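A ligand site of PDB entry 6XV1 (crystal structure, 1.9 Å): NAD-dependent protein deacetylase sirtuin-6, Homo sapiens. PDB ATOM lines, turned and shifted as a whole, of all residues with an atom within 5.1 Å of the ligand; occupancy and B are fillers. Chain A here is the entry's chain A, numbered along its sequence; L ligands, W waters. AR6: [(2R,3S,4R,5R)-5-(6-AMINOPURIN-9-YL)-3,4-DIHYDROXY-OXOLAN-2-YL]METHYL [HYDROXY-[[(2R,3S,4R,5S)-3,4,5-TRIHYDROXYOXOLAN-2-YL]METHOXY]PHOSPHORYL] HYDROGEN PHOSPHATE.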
ATOM      1  N   GLU A  16     -22.873  -7.924 -16.518  1.00  0.00           N
ATOM      2  CA  GLU A  16     -24.214  -7.324 -16.609  1.00  0.00           C
ATOM      3  C   GLU A  16     -25.253  -8.419 -16.326  1.00  0.00           C
ATOM      4  O   GLU A  16     -24.995  -9.547 -16.696  1.00  0.00           O
ATOM      5  CB  GLU A  16     -24.396  -6.729 -17.999  1.00  0.00           C
ATOM      6  CG  GLU A  16     -23.654  -5.433 -18.238  1.00  0.00           C
ATOM      7  CD  GLU A  16     -23.924  -4.805 -19.594  1.00  0.00           C
ATOM      8  OE1 GLU A  16     -24.192  -5.534 -20.516  1.00  0.00           O
ATOM      9  OE2 GLU A  16     -23.868  -3.615 -19.698  1.00  0.00           O
ATOM     10  N   THR A  45     -29.045   9.586  -9.771  1.00  0.00           N
ATOM     11  CA  THR A  45     -28.611   9.153 -11.135  1.00  0.00           C
ATOM     12  C   THR A  45     -27.094   9.140 -11.269  1.00  0.00           C
ATOM     13  O   THR A  45     -26.408   9.936 -10.570  1.00  0.00           O
ATOM     14  CB  THR A  45     -29.132  10.055 -12.265  1.00  0.00           C
ATOM     15  OG1 THR A  45     -28.653  11.375 -12.068  1.00  0.00           O
ATOM     16  CG2 THR A  45     -30.625  10.035 -12.379  1.00  0.00           C
ATOM     17  N   GLY A  46     -26.574   8.271 -12.166  1.00  0.00           N
ATOM     18  CA  GLY A  46     -25.129   8.133 -12.438  1.00  0.00           C
ATOM     19  C   GLY A  46     -24.941   7.932 -13.905  1.00  0.00           C
ATOM     20  O   GLY A  46     -25.975   7.988 -14.626  1.00  0.00           O
ATOM     21  N   ALA A  47     -23.720   7.666 -14.281  1.00  0.00           N
ATOM     22  CA  ALA A  47     -23.199   7.684 -15.659  1.00  0.00           C
ATOM     23  C   ALA A  47     -23.990   6.711 -16.516  1.00  0.00           C
ATOM     24  O   ALA A  47     -24.077   7.047 -17.707  1.00  0.00           O
ATOM     25  CB  ALA A  47     -21.740   7.348 -15.722  1.00  0.00           C
ATOM     26  N   GLY A  48     -24.741   5.774 -15.965  1.00  0.00           N
ATOM     27  CA  GLY A  48     -25.515   4.791 -16.767  1.00  0.00           C
ATOM     28  C   GLY A  48     -26.733   5.376 -17.459  1.00  0.00           C
ATOM     29  O   GLY A  48     -27.083   4.964 -18.624  1.00  0.00           O
ATOM     30  N   THR A  51     -25.334   6.716 -21.120  1.00  0.00           N
ATOM     31  CA  THR A  51     -24.672   5.776 -22.097  1.00  0.00           C
ATOM     32  C   THR A  51     -25.428   5.825 -23.434  1.00  0.00           C
ATOM     33  O   THR A  51     -24.814   5.738 -24.476  1.00  0.00           O
ATOM     34  CB  THR A  51     -24.413   4.375 -21.544  1.00  0.00           C
ATOM     35  OG1 THR A  51     -25.640   3.794 -21.097  1.00  0.00           O
ATOM     36  CG2 THR A  51     -23.302   4.437 -20.501  1.00  0.00           C
ATOM     37  N   ALA A  52     -26.742   5.878 -23.386  1.00  0.00           N
ATOM     38  CA  ALA A  52     -27.686   5.765 -24.552  1.00  0.00           C
ATOM     39  C   ALA A  52     -27.724   7.054 -25.343  1.00  0.00           C
ATOM     40  O   ALA A  52     -28.358   7.046 -26.473  1.00  0.00           O
ATOM     41  CB  ALA A  52     -29.010   5.309 -24.083  1.00  0.00           C
ATOM     42  N   ASP A  57     -19.848   5.196 -19.557  1.00  0.00           N
ATOM     43  CA  ASP A  57     -19.916   5.193 -18.067  1.00  0.00           C
ATOM     44  C   ASP A  57     -18.483   5.004 -17.547  1.00  0.00           C
ATOM     45  O   ASP A  57     -17.551   5.229 -18.360  1.00  0.00           O
ATOM     46  CB  ASP A  57     -20.980   4.236 -17.593  1.00  0.00           C
ATOM     47  CG  ASP A  57     -20.659   2.787 -17.964  1.00  0.00           C
ATOM     48  OD1 ASP A  57     -19.526   2.520 -18.307  1.00  0.00           O
ATOM     49  OD2 ASP A  57     -21.532   1.962 -17.769  1.00  0.00           O
ATOM     50  N   PHE A  58     -18.280   4.883 -16.234  1.00  0.00           N
ATOM     51  CA  PHE A  58     -16.947   4.625 -15.633  1.00  0.00           C
ATOM     52  C   PHE A  58     -16.661   3.140 -15.461  1.00  0.00           C
ATOM     53  O   PHE A  58     -15.546   2.775 -15.776  1.00  0.00           O
ATOM     54  CB  PHE A  58     -16.860   5.429 -14.316  1.00  0.00           C
ATOM     55  CG  PHE A  58     -16.905   6.901 -14.572  1.00  0.00           C
ATOM     56  CD1 PHE A  58     -15.768   7.598 -14.897  1.00  0.00           C
ATOM     57  CD2 PHE A  58     -18.100   7.621 -14.490  1.00  0.00           C
ATOM     58  CE1 PHE A  58     -15.813   8.953 -15.207  1.00  0.00           C
ATOM     59  CE2 PHE A  58     -18.120   8.985 -14.732  1.00  0.00           C
ATOM     60  CZ  PHE A  58     -16.968   9.657 -15.115  1.00  0.00           C
ATOM     61  N   ARG A  59     -17.585   2.331 -14.932  1.00  0.00           N
ATOM     62  CA  ARG A  59     -17.238   0.978 -14.440  1.00  0.00           C
ATOM     63  C   ARG A  59     -18.046  -0.053 -15.177  1.00  0.00           C
ATOM     64  O   ARG A  59     -18.037  -1.190 -14.833  1.00  0.00           O
ATOM     65  CB  ARG A  59     -17.422   0.899 -12.949  1.00  0.00           C
ATOM     66  CG  ARG A  59     -16.609   2.000 -12.281  1.00  0.00           C
ATOM     67  CD  ARG A  59     -16.689   1.845 -10.766  1.00  0.00           C
ATOM     68  NE  ARG A  59     -16.024   2.931 -10.147  1.00  0.00           N
ATOM     69  CZ  ARG A  59     -16.411   4.224 -10.096  1.00  0.00           C
ATOM     70  NH1 ARG A  59     -17.531   4.697 -10.655  1.00  0.00           N
ATOM     71  NH2 ARG A  59     -15.611   5.083  -9.511  1.00  0.00           N
ATOM     72  N   GLY A  60     -18.726   0.365 -16.239  1.00  0.00           N
ATOM     73  CA  GLY A  60     -19.392  -0.610 -17.113  1.00  0.00           C
ATOM     74  C   GLY A  60     -18.384  -1.395 -17.938  1.00  0.00           C
ATOM     75  O   GLY A  60     -17.187  -1.134 -17.943  1.00  0.00           O
ATOM     76  N   TRP A  65     -12.897   3.837 -16.661  1.00  0.00           N
ATOM     77  CA  TRP A  65     -12.001   3.158 -15.696  1.00  0.00           C
ATOM     78  C   TRP A  65     -11.806   1.688 -16.127  1.00  0.00           C
ATOM     79  O   TRP A  65     -10.667   1.183 -16.128  1.00  0.00           O
ATOM     80  CB  TRP A  65     -12.543   3.230 -14.252  1.00  0.00           C
ATOM     81  CG  TRP A  65     -12.796   4.593 -13.667  1.00  0.00           C
ATOM     82  CD1 TRP A  65     -13.567   4.833 -12.551  1.00  0.00           C
ATOM     83  CD2 TRP A  65     -12.193   5.858 -13.982  1.00  0.00           C
ATOM     84  NE1 TRP A  65     -13.578   6.174 -12.228  1.00  0.00           N
ATOM     85  CE2 TRP A  65     -12.733   6.833 -13.077  1.00  0.00           C
ATOM     86  CE3 TRP A  65     -11.289   6.288 -14.962  1.00  0.00           C
ATOM     87  CZ2 TRP A  65     -12.419   8.180 -13.167  1.00  0.00           C
ATOM     88  CZ3 TRP A  65     -10.974   7.639 -15.042  1.00  0.00           C
ATOM     89  CH2 TRP A  65     -11.546   8.562 -14.157  1.00  0.00           C
ATOM     90  N   GLN A 107     -24.570  12.317  -9.671  1.00  0.00           N
ATOM     91  CA  GLN A 107     -23.132  12.264  -9.694  1.00  0.00           C
ATOM     92  C   GLN A 107     -22.612  12.752 -11.026  1.00  0.00           C
ATOM     93  O   GLN A 107     -21.413  12.699 -11.187  1.00  0.00           O
ATOM     94  CB  GLN A 107     -22.767  10.802  -9.434  1.00  0.00           C
ATOM     95  CG  GLN A 107     -23.097  10.452  -7.996  1.00  0.00           C
ATOM     96  CD  GLN A 107     -22.862   9.019  -7.663  1.00  0.00           C
ATOM     97  OE1 GLN A 107     -21.740   8.574  -7.447  1.00  0.00           O
ATOM     98  NE2 GLN A 107     -23.982   8.291  -7.607  1.00  0.00           N
ATOM     99  N   ASN A 108     -23.501  12.925 -12.013  1.00  0.00           N
ATOM    100  CA  ASN A 108     -23.039  13.082 -13.411  1.00  0.00           C
ATOM    101  C   ASN A 108     -22.514  14.522 -13.532  1.00  0.00           C
ATOM    102  O   ASN A 108     -23.124  15.519 -13.011  1.00  0.00           O
ATOM    103  CB  ASN A 108     -24.111  12.746 -14.457  1.00  0.00           C
ATOM    104  CG  ASN A 108     -24.511  11.299 -14.405  1.00  0.00           C
ATOM    105  OD1 ASN A 108     -23.748  10.479 -13.885  1.00  0.00           O
ATOM    106  ND2 ASN A 108     -25.656  10.928 -14.968  1.00  0.00           N
ATOM    107  N   HIS A 127     -20.816  16.028  -8.138  1.00  0.00           N
ATOM    108  CA  HIS A 127     -19.445  15.864  -8.691  1.00  0.00           C
ATOM    109  C   HIS A 127     -19.097  17.048  -9.574  1.00  0.00           C
ATOM    110  O   HIS A 127     -17.988  17.021 -10.192  1.00  0.00           O
ATOM    111  CB  HIS A 127     -19.318  14.480  -9.336  1.00  0.00           C
ATOM    112  CG  HIS A 127     -19.474  13.374  -8.326  1.00  0.00           C
ATOM    113  ND1 HIS A 127     -19.508  12.002  -8.696  1.00  0.00           N
ATOM    114  CD2 HIS A 127     -19.535  13.375  -6.978  1.00  0.00           C
ATOM    115  CE1 HIS A 127     -19.730  11.298  -7.639  1.00  0.00           C
ATOM    116  NE2 HIS A 127     -19.735  12.071  -6.598  1.00  0.00           N
ATOM    117  N   TRP A 182     -10.380  13.813  -7.281  1.00  0.00           N
ATOM    118  CA  TRP A 182     -10.470  12.711  -6.303  1.00  0.00           C
ATOM    119  C   TRP A 182     -10.431  13.263  -4.878  1.00  0.00           C
ATOM    120  O   TRP A 182     -11.311  12.881  -4.134  1.00  0.00           O
ATOM    121  CB  TRP A 182      -9.369  11.676  -6.537  1.00  0.00           C
ATOM    122  CG  TRP A 182      -9.661  10.784  -7.707  1.00  0.00           C
ATOM    123  CD1 TRP A 182      -9.064  10.840  -8.948  1.00  0.00           C
ATOM    124  CD2 TRP A 182     -10.674   9.766  -7.787  1.00  0.00           C
ATOM    125  NE1 TRP A 182      -9.619   9.886  -9.781  1.00  0.00           N
ATOM    126  CE2 TRP A 182     -10.612   9.220  -9.101  1.00  0.00           C
ATOM    127  CE3 TRP A 182     -11.613   9.243  -6.888  1.00  0.00           C
ATOM    128  CZ2 TRP A 182     -11.457   8.183  -9.519  1.00  0.00           C
ATOM    129  CZ3 TRP A 182     -12.450   8.222  -7.302  1.00  0.00           C
ATOM    130  CH2 TRP A 182     -12.363   7.679  -8.599  1.00  0.00           C
ATOM    131  N   GLY A 208     -28.676   3.715 -13.049  1.00  0.00           N
ATOM    132  CA  GLY A 208     -27.378   3.731 -13.763  1.00  0.00           C
ATOM    133  C   GLY A 208     -26.264   4.316 -12.898  1.00  0.00           C
ATOM    134  O   GLY A 208     -25.490   5.109 -13.443  1.00  0.00           O
ATOM    135  N   THR A 209     -26.261   4.044 -11.578  1.00  0.00           N
ATOM    136  CA  THR A 209     -25.025   4.154 -10.710  1.00  0.00           C
ATOM    137  C   THR A 209     -24.725   2.816 -10.002  1.00  0.00           C
ATOM    138  O   THR A 209     -25.652   2.125  -9.558  1.00  0.00           O
ATOM    139  CB  THR A 209     -25.172   5.296  -9.706  1.00  0.00           C
ATOM    140  OG1 THR A 209     -24.113   5.292  -8.739  1.00  0.00           O
ATOM    141  CG2 THR A 209     -26.502   5.295  -9.014  1.00  0.00           C
ATOM    142  N   SER A 210     -23.423   2.505  -9.935  1.00  0.00           N
ATOM    143  CA  SER A 210     -22.867   1.354  -9.224  1.00  0.00           C
ATOM    144  C   SER A 210     -22.868   1.654  -7.702  1.00  0.00           C
ATOM    145  O   SER A 210     -22.606   0.728  -6.912  1.00  0.00           O
ATOM    146  CB  SER A 210     -21.460   0.973  -9.768  1.00  0.00           C
ATOM    147  OG  SER A 210     -20.445   1.972  -9.574  1.00  0.00           O
ATOM    148  N   LEU A 211     -23.025   2.894  -7.311  1.00  0.00           N
ATOM    149  CA  LEU A 211     -23.083   3.297  -5.851  1.00  0.00           C
ATOM    150  C   LEU A 211     -21.780   2.989  -5.088  1.00  0.00           C
ATOM    151  O   LEU A 211     -21.827   2.770  -3.822  1.00  0.00           O
ATOM    152  CB  LEU A 211     -24.297   2.627  -5.202  1.00  0.00           C
ATOM    153  CG  LEU A 211     -25.687   2.902  -5.748  1.00  0.00           C
ATOM    154  CD1 LEU A 211     -26.769   2.019  -5.084  1.00  0.00           C
ATOM    155  CD2 LEU A 211     -26.073   4.413  -5.605  1.00  0.00           C
ATOM    156  N   GLN A 212     -20.628   3.127  -5.729  1.00  0.00           N
ATOM    157  CA  GLN A 212     -19.336   2.773  -5.065  1.00  0.00           C
ATOM    158  C   GLN A 212     -18.674   3.999  -4.421  1.00  0.00           C
ATOM    159  O   GLN A 212     -17.628   3.780  -3.846  1.00  0.00           O
ATOM    160  CB  GLN A 212     -18.386   2.133  -6.073  1.00  0.00           C
ATOM    161  CG  GLN A 212     -18.998   1.011  -6.912  1.00  0.00           C
ATOM    162  CD  GLN A 212     -18.007   0.048  -7.499  1.00  0.00           C
ATOM    163  OE1 GLN A 212     -16.977  -0.250  -6.873  1.00  0.00           O
ATOM    164  NE2 GLN A 212     -18.310  -0.450  -8.714  1.00  0.00           N
ATOM    165  N   ILE A 213     -19.166   5.199  -4.687  1.00  0.00           N
ATOM    166  CA  ILE A 213     -18.495   6.434  -4.208  1.00  0.00           C
ATOM    167  C   ILE A 213     -19.172   6.974  -2.955  1.00  0.00           C
ATOM    168  O   ILE A 213     -20.376   7.087  -2.955  1.00  0.00           O
ATOM    169  CB  ILE A 213     -18.456   7.502  -5.305  1.00  0.00           C
ATOM    170  CG1 ILE A 213     -17.764   7.009  -6.566  1.00  0.00           C
ATOM    171  CG2 ILE A 213     -17.807   8.774  -4.783  1.00  0.00           C
ATOM    172  CD1 ILE A 213     -16.270   7.091  -6.506  1.00  0.00           C
ATOM    173  N   VAL A 233     -32.026   0.572 -10.040  1.00  0.00           N
ATOM    174  CA  VAL A 233     -32.147   0.175 -11.477  1.00  0.00           C
ATOM    175  C   VAL A 233     -30.761   0.262 -12.101  1.00  0.00           C
ATOM    176  O   VAL A 233     -30.151   1.357 -12.035  1.00  0.00           O
ATOM    177  CB  VAL A 233     -33.155   1.059 -12.211  1.00  0.00           C
ATOM    178  CG1 VAL A 233     -33.290   0.679 -13.684  1.00  0.00           C
ATOM    179  CG2 VAL A 233     -34.508   1.073 -11.553  1.00  0.00           C
ATOM    180  N   ASN A 234     -30.211  -0.886 -12.569  1.00  0.00           N
ATOM    181  CA  ASN A 234     -28.770  -0.958 -12.908  1.00  0.00           C
ATOM    182  C   ASN A 234     -28.412  -2.276 -13.620  1.00  0.00           C
ATOM    183  O   ASN A 234     -28.928  -3.334 -13.135  1.00  0.00           O
ATOM    184  CB  ASN A 234     -27.847  -0.866 -11.677  1.00  0.00           C
ATOM    185  CG  ASN A 234     -26.534  -0.204 -12.112  1.00  0.00           C
ATOM    186  OD1 ASN A 234     -26.574   0.906 -12.613  1.00  0.00           O
ATOM    187  ND2 ASN A 234     -25.381  -0.827 -11.901  1.00  0.00           N
ATOM    188  N   LEU A 235     -27.671  -2.224 -14.762  1.00  0.00           N
ATOM    189  CA  LEU A 235     -27.299  -3.482 -15.477  1.00  0.00           C
ATOM    190  C   LEU A 235     -26.338  -4.374 -14.637  1.00  0.00           C
ATOM    191  O   LEU A 235     -26.488  -5.634 -14.645  1.00  0.00           O
ATOM    192  CB  LEU A 235     -26.712  -3.166 -16.874  1.00  0.00           C
ATOM    193  CG  LEU A 235     -27.823  -2.770 -17.879  1.00  0.00           C
ATOM    194  CD1 LEU A 235     -27.285  -2.057 -19.080  1.00  0.00           C
ATOM    195  CD2 LEU A 235     -28.593  -4.011 -18.331  1.00  0.00           C
ATOM    196  N   GLN A 236     -25.469  -3.775 -13.829  1.00  0.00           N
ATOM    197  CA  GLN A 236     -24.396  -4.442 -13.043  1.00  0.00           C
ATOM    198  C   GLN A 236     -24.891  -4.471 -11.623  1.00  0.00           C
ATOM    199  O   GLN A 236     -25.764  -3.684 -11.246  1.00  0.00           O
ATOM    200  CB  GLN A 236     -23.069  -3.692 -13.104  1.00  0.00           C
ATOM    201  CG  GLN A 236     -22.292  -3.900 -14.372  1.00  0.00           C
ATOM    202  CD  GLN A 236     -21.036  -3.053 -14.425  1.00  0.00           C
ATOM    203  OE1 GLN A 236     -20.901  -2.002 -13.740  1.00  0.00           O
ATOM    204  NE2 GLN A 236     -20.063  -3.472 -15.248  1.00  0.00           N
ATOM    205  N   PRO A 237     -24.350  -5.405 -10.837  1.00  0.00           N
ATOM    206  CA  PRO A 237     -24.444  -5.351  -9.385  1.00  0.00           C
ATOM    207  C   PRO A 237     -23.992  -3.969  -8.918  1.00  0.00           C
ATOM    208  O   PRO A 237     -23.224  -3.296  -9.590  1.00  0.00           O
ATOM    209  CB  PRO A 237     -23.530  -6.441  -8.843  1.00  0.00           C
ATOM    210  CG  PRO A 237     -23.105  -7.253 -10.058  1.00  0.00           C
ATOM    211  CD  PRO A 237     -23.460  -6.503 -11.307  1.00  0.00           C
ATOM    212  N   GLY A 250     -32.023  -3.988 -16.172  1.00  0.00           N
ATOM    213  CA  GLY A 250     -32.466  -3.651 -17.539  1.00  0.00           C
ATOM    214  C   GLY A 250     -31.972  -2.279 -17.952  1.00  0.00           C
ATOM    215  O   GLY A 250     -31.466  -1.582 -17.063  1.00  0.00           O
ATOM    216  N   TYR A 251     -31.991  -1.973 -19.250  1.00  0.00           N
ATOM    217  CA  TYR A 251     -31.721  -0.614 -19.756  1.00  0.00           C
ATOM    218  C   TYR A 251     -32.674   0.385 -19.059  1.00  0.00           C
ATOM    219  O   TYR A 251     -33.848   0.108 -19.061  1.00  0.00           O
ATOM    220  CB  TYR A 251     -31.803  -0.565 -21.273  1.00  0.00           C
ATOM    221  CG  TYR A 251     -30.783  -1.472 -21.895  1.00  0.00           C
ATOM    222  CD1 TYR A 251     -29.423  -1.196 -21.833  1.00  0.00           C
ATOM    223  CD2 TYR A 251     -31.161  -2.632 -22.528  1.00  0.00           C
ATOM    224  CE1 TYR A 251     -28.522  -1.994 -22.498  1.00  0.00           C
ATOM    225  CE2 TYR A 251     -30.259  -3.530 -23.051  1.00  0.00           C
ATOM    226  CZ  TYR A 251     -28.921  -3.194 -23.093  1.00  0.00           C
ATOM    227  OH  TYR A 251     -28.077  -4.132 -23.636  1.00  0.00           O
ATOM    228  N   VAL A 252     -32.141   1.471 -18.496  1.00  0.00           N
ATOM    229  CA  VAL A 252     -32.912   2.507 -17.795  1.00  0.00           C
ATOM    230  C   VAL A 252     -33.917   3.106 -18.737  1.00  0.00           C
ATOM    231  O   VAL A 252     -35.030   3.176 -18.337  1.00  0.00           O
ATOM    232  CB  VAL A 252     -32.082   3.563 -17.113  1.00  0.00           C
ATOM    233  CG1 VAL A 252     -31.557   2.968 -15.858  1.00  0.00           C
ATOM    234  CG2 VAL A 252     -30.955   4.151 -17.998  1.00  0.00           C
HETATM  235  N1  AR6 L   1     -29.173   1.120 -18.253  1.00  0.00           N
HETATM  236  C2  AR6 L   1     -28.915   0.737 -16.993  1.00  0.00           C
HETATM  237  N3  AR6 L   1     -27.744   0.648 -16.365  1.00  0.00           N
HETATM  238  C4  AR6 L   1     -26.758   1.066 -17.159  1.00  0.00           C
HETATM  239  C5  AR6 L   1     -26.875   1.509 -18.470  1.00  0.00           C
HETATM  240  C6  AR6 L   1     -28.155   1.538 -19.050  1.00  0.00           C
HETATM  241  N6  AR6 L   1     -28.405   1.969 -20.307  1.00  0.00           N
HETATM  242  N7  AR6 L   1     -25.635   1.888 -18.943  1.00  0.00           N
HETATM  243  C8  AR6 L   1     -24.843   1.744 -17.920  1.00  0.00           C
HETATM  244  N9  AR6 L   1     -25.438   1.197 -16.834  1.00  0.00           N
HETATM  245  PA  AR6 L   1     -20.504   3.842 -12.758  1.00  0.00           P
HETATM  246  PB  AR6 L   1     -21.331   6.255 -11.270  1.00  0.00           P
HETATM  247  C1' AR6 L   1     -24.886   0.955 -15.474  1.00  0.00           C
HETATM  248  O1A AR6 L   1     -19.808   3.419 -11.514  1.00  0.00           O
HETATM  249  O1B AR6 L   1     -22.203   7.338 -11.740  1.00  0.00           O
HETATM  250  C1D AR6 L   1     -16.562   8.023 -10.939  1.00  0.00           C
HETATM  251  O1D AR6 L   1     -15.275   8.164 -10.431  1.00  0.00           O
HETATM  252  C2' AR6 L   1     -23.591   0.194 -15.416  1.00  0.00           C
HETATM  253  O2' AR6 L   1     -23.897  -1.159 -15.389  1.00  0.00           O
HETATM  254  O2A AR6 L   1     -19.920   3.638 -14.107  1.00  0.00           O
HETATM  255  O2B AR6 L   1     -21.935   5.239 -10.357  1.00  0.00           O
HETATM  256  C2D AR6 L   1     -17.145   9.416 -11.337  1.00  0.00           C
HETATM  257  O2D AR6 L   1     -16.740  10.437 -10.464  1.00  0.00           O
HETATM  258  C3' AR6 L   1     -22.844   0.762 -14.192  1.00  0.00           C
HETATM  259  O3' AR6 L   1     -23.046  -0.196 -13.186  1.00  0.00           O
HETATM  260  O3A AR6 L   1     -20.829   5.444 -12.646  1.00  0.00           O
HETATM  261  C3D AR6 L   1     -18.649   9.266 -11.135  1.00  0.00           C
HETATM  262  O3D AR6 L   1     -19.288  10.512 -10.817  1.00  0.00           O
HETATM  263  C4' AR6 L   1     -23.627   2.036 -13.897  1.00  0.00           C
HETATM  264  O4' AR6 L   1     -24.602   2.206 -14.936  1.00  0.00           O
HETATM  265  C4D AR6 L   1     -18.659   8.344  -9.922  1.00  0.00           C
HETATM  266  O4D AR6 L   1     -17.478   7.501  -9.989  1.00  0.00           O
HETATM  267  C5' AR6 L   1     -22.763   3.244 -13.886  1.00  0.00           C
HETATM  268  O5' AR6 L   1     -21.891   3.162 -12.725  1.00  0.00           O
HETATM  269  C5D AR6 L   1     -19.903   7.532  -9.733  1.00  0.00           C
HETATM  270  O5D AR6 L   1     -19.913   6.640 -10.890  1.00  0.00           O
HETATM  271  O   HOH W   1     -21.198   9.950 -12.693  1.00  0.00           O
HETATM  272  O   HOH W   2     -28.602   5.279 -21.021  1.00  0.00           O
HETATM  273  O   HOH W   3     -20.340   4.265  -8.538  1.00  0.00           O
HETATM  274  O   HOH W   4     -22.226  -0.040 -19.309  1.00  0.00           O
HETATM  275  O   HOH W   5     -30.940   3.110 -21.518  1.00  0.00           O
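An oxygen (O3') of the ligand sits at hydrogen-bond distance from the side-chain amide oxygen (OE1) of Gln 236, 2.9 Å away.
N of Val 252 sits at hydrogen-bond distance from N1 of the ligand, 3.0 Å away.
An oxygen (O2A) of the ligand lies within hydrogen-bond range of the backbone NH of Arg 59 (2.8 Å).
The backbone carbonyl oxygen (O) of Gln 107 is in hydrogen-bond range of an oxygen (O3D) of the ligand (3.1 Å).
The backbone NH of Gln 236 sits close to an oxygen (O2') of the ligand (3.4 Å).
The backbone NH of Ser 210 is in hydrogen-bond range of an oxygen (O2B) of the ligand, at 3.1 Å.
The backbone NH of Phe 58 lies within hydrogen-bond range of an oxygen (O2A) of the ligand, at 3.0 Å.
A ring nitrogen (ND1) of His 127 sits at hydrogen-bond distance from an oxygen (O3D) of the ligand, 2.6 Å away.
O2B of the ligand is in hydrogen-bond range of OG1 of Thr 209, at 2.7 Å.
O1A of the ligand is in salt-bridge range of NH1 of Arg 59 (2.7 Å).
ND2 of Asn 234 lies within hydrogen-bond range of O3' of the ligand, 2.7 Å away.
The side-chain hydroxyl (OG) of Ser 210 is in hydrogen-bond range of an oxygen (O1A) of the ligand.
O1B of the ligand sits at hydrogen-bond distance from N of Ala 47.
The side-chain hydroxyl (OG1) of Thr 51 lies within hydrogen-bond range of a nitrogen (N7) of the ligand (2.9 Å).
The backbone NH (N) of Leu 235 is in hydrogen-bond range of a nitrogen (N3) of the ligand, at 3.3 Å.
NE1 of Trp 65 is in hydrogen-bond range of O1D of the ligand.
N of Trp 65 sits at hydrogen-bond distance from O of Phe 58 (3.0 Å).
The backbone carbonyl oxygen of Gln 236 lies within hydrogen-bond range of the side-chain amide nitrogen of Asn 234 (3.0 Å).
The backbone NH (N) of Gly 208 sits at hydrogen-bond distance from the backbone carbonyl oxygen (O) of Val 233 (3.0 Å).
The side-chain amide nitrogen (NE2) of Gln 107 lies within hydrogen-bond range of the side-chain hydroxyl (OG1) of Thr 209 (3.2 Å).
A ring nitrogen (ND1) of His 127 is in hydrogen-bond range of the backbone carbonyl oxygen (O) of Gln 107, at 3.2 Å.
The backbone NH (N) of Gly 48 lies within hydrogen-bond range of the backbone carbonyl oxygen (O) of Gly 208 (2.7 Å).
The backbone carbonyl oxygen (O) of Arg 59 sits at hydrogen-bond distance from the side-chain amide nitrogen (NE2) of Gln 236, 3.1 Å away.
The backbone NH (N) of Gln 107 sits at hydrogen-bond distance from the backbone carbonyl oxygen (O) of Thr 45, at 3.1 Å.
A nitrogen (N7) of the ligand lies close to the backbone carbonyl oxygen (O) of Gly 48, at 3.4 Å.
O of Gly 208 sits close to O4' of the ligand (3.4 Å).
Residues that only touch the ligand: Gly 46, Asp 57, Tyr 251, Gly 250, Ile 213, Trp 182 and Leu 211.
Hydrophobic or aromatic side chains within 4 Å of the ligand: Ala 47, Phe 58, Trp 65, His 127, Trp 182, Ile 213, Leu 235, Tyr 251 and Val 252.
22 residues have an atom within 4 Å of the ligand: Gly 46, Ala 47, Gly 48, Thr 51, Asp 57, Phe 58, Arg 59, Trp 65, Gln 107, His 127, Trp 182, Gly 208, Thr 209, Ser 210, Leu 211, Ile 213, Asn 234, Leu 235, Gln 236, Gly 250, Tyr 251 and Val 252.
The nearest printed residue that does not touch the ligand is Gly 60 (4.1 Å).
Water W3 lies within hydrogen-bond range of the side-chain hydroxyl (OG) of Ser 210 (2.5 Å), an oxygen (O2B) of the ligand (2.6 Å), the backbone NH (N) of Gln 212 (3.0 Å) and the backbone NH (N) of Leu 211 (3.3 Å).
Water W1 lies within hydrogen-bond range of O3D of the ligand (2.7 Å), OD1 of Asn 108 (2.9 Å) and O of Gln 107 (3.1 Å).
Water W2 lies within hydrogen-bond range of O of Gly 48 (2.9 Å), N of Ala 52 (3.1 Å), OG1 of Thr 51 (3.3 Å) and N6 of the ligand (3.4 Å).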
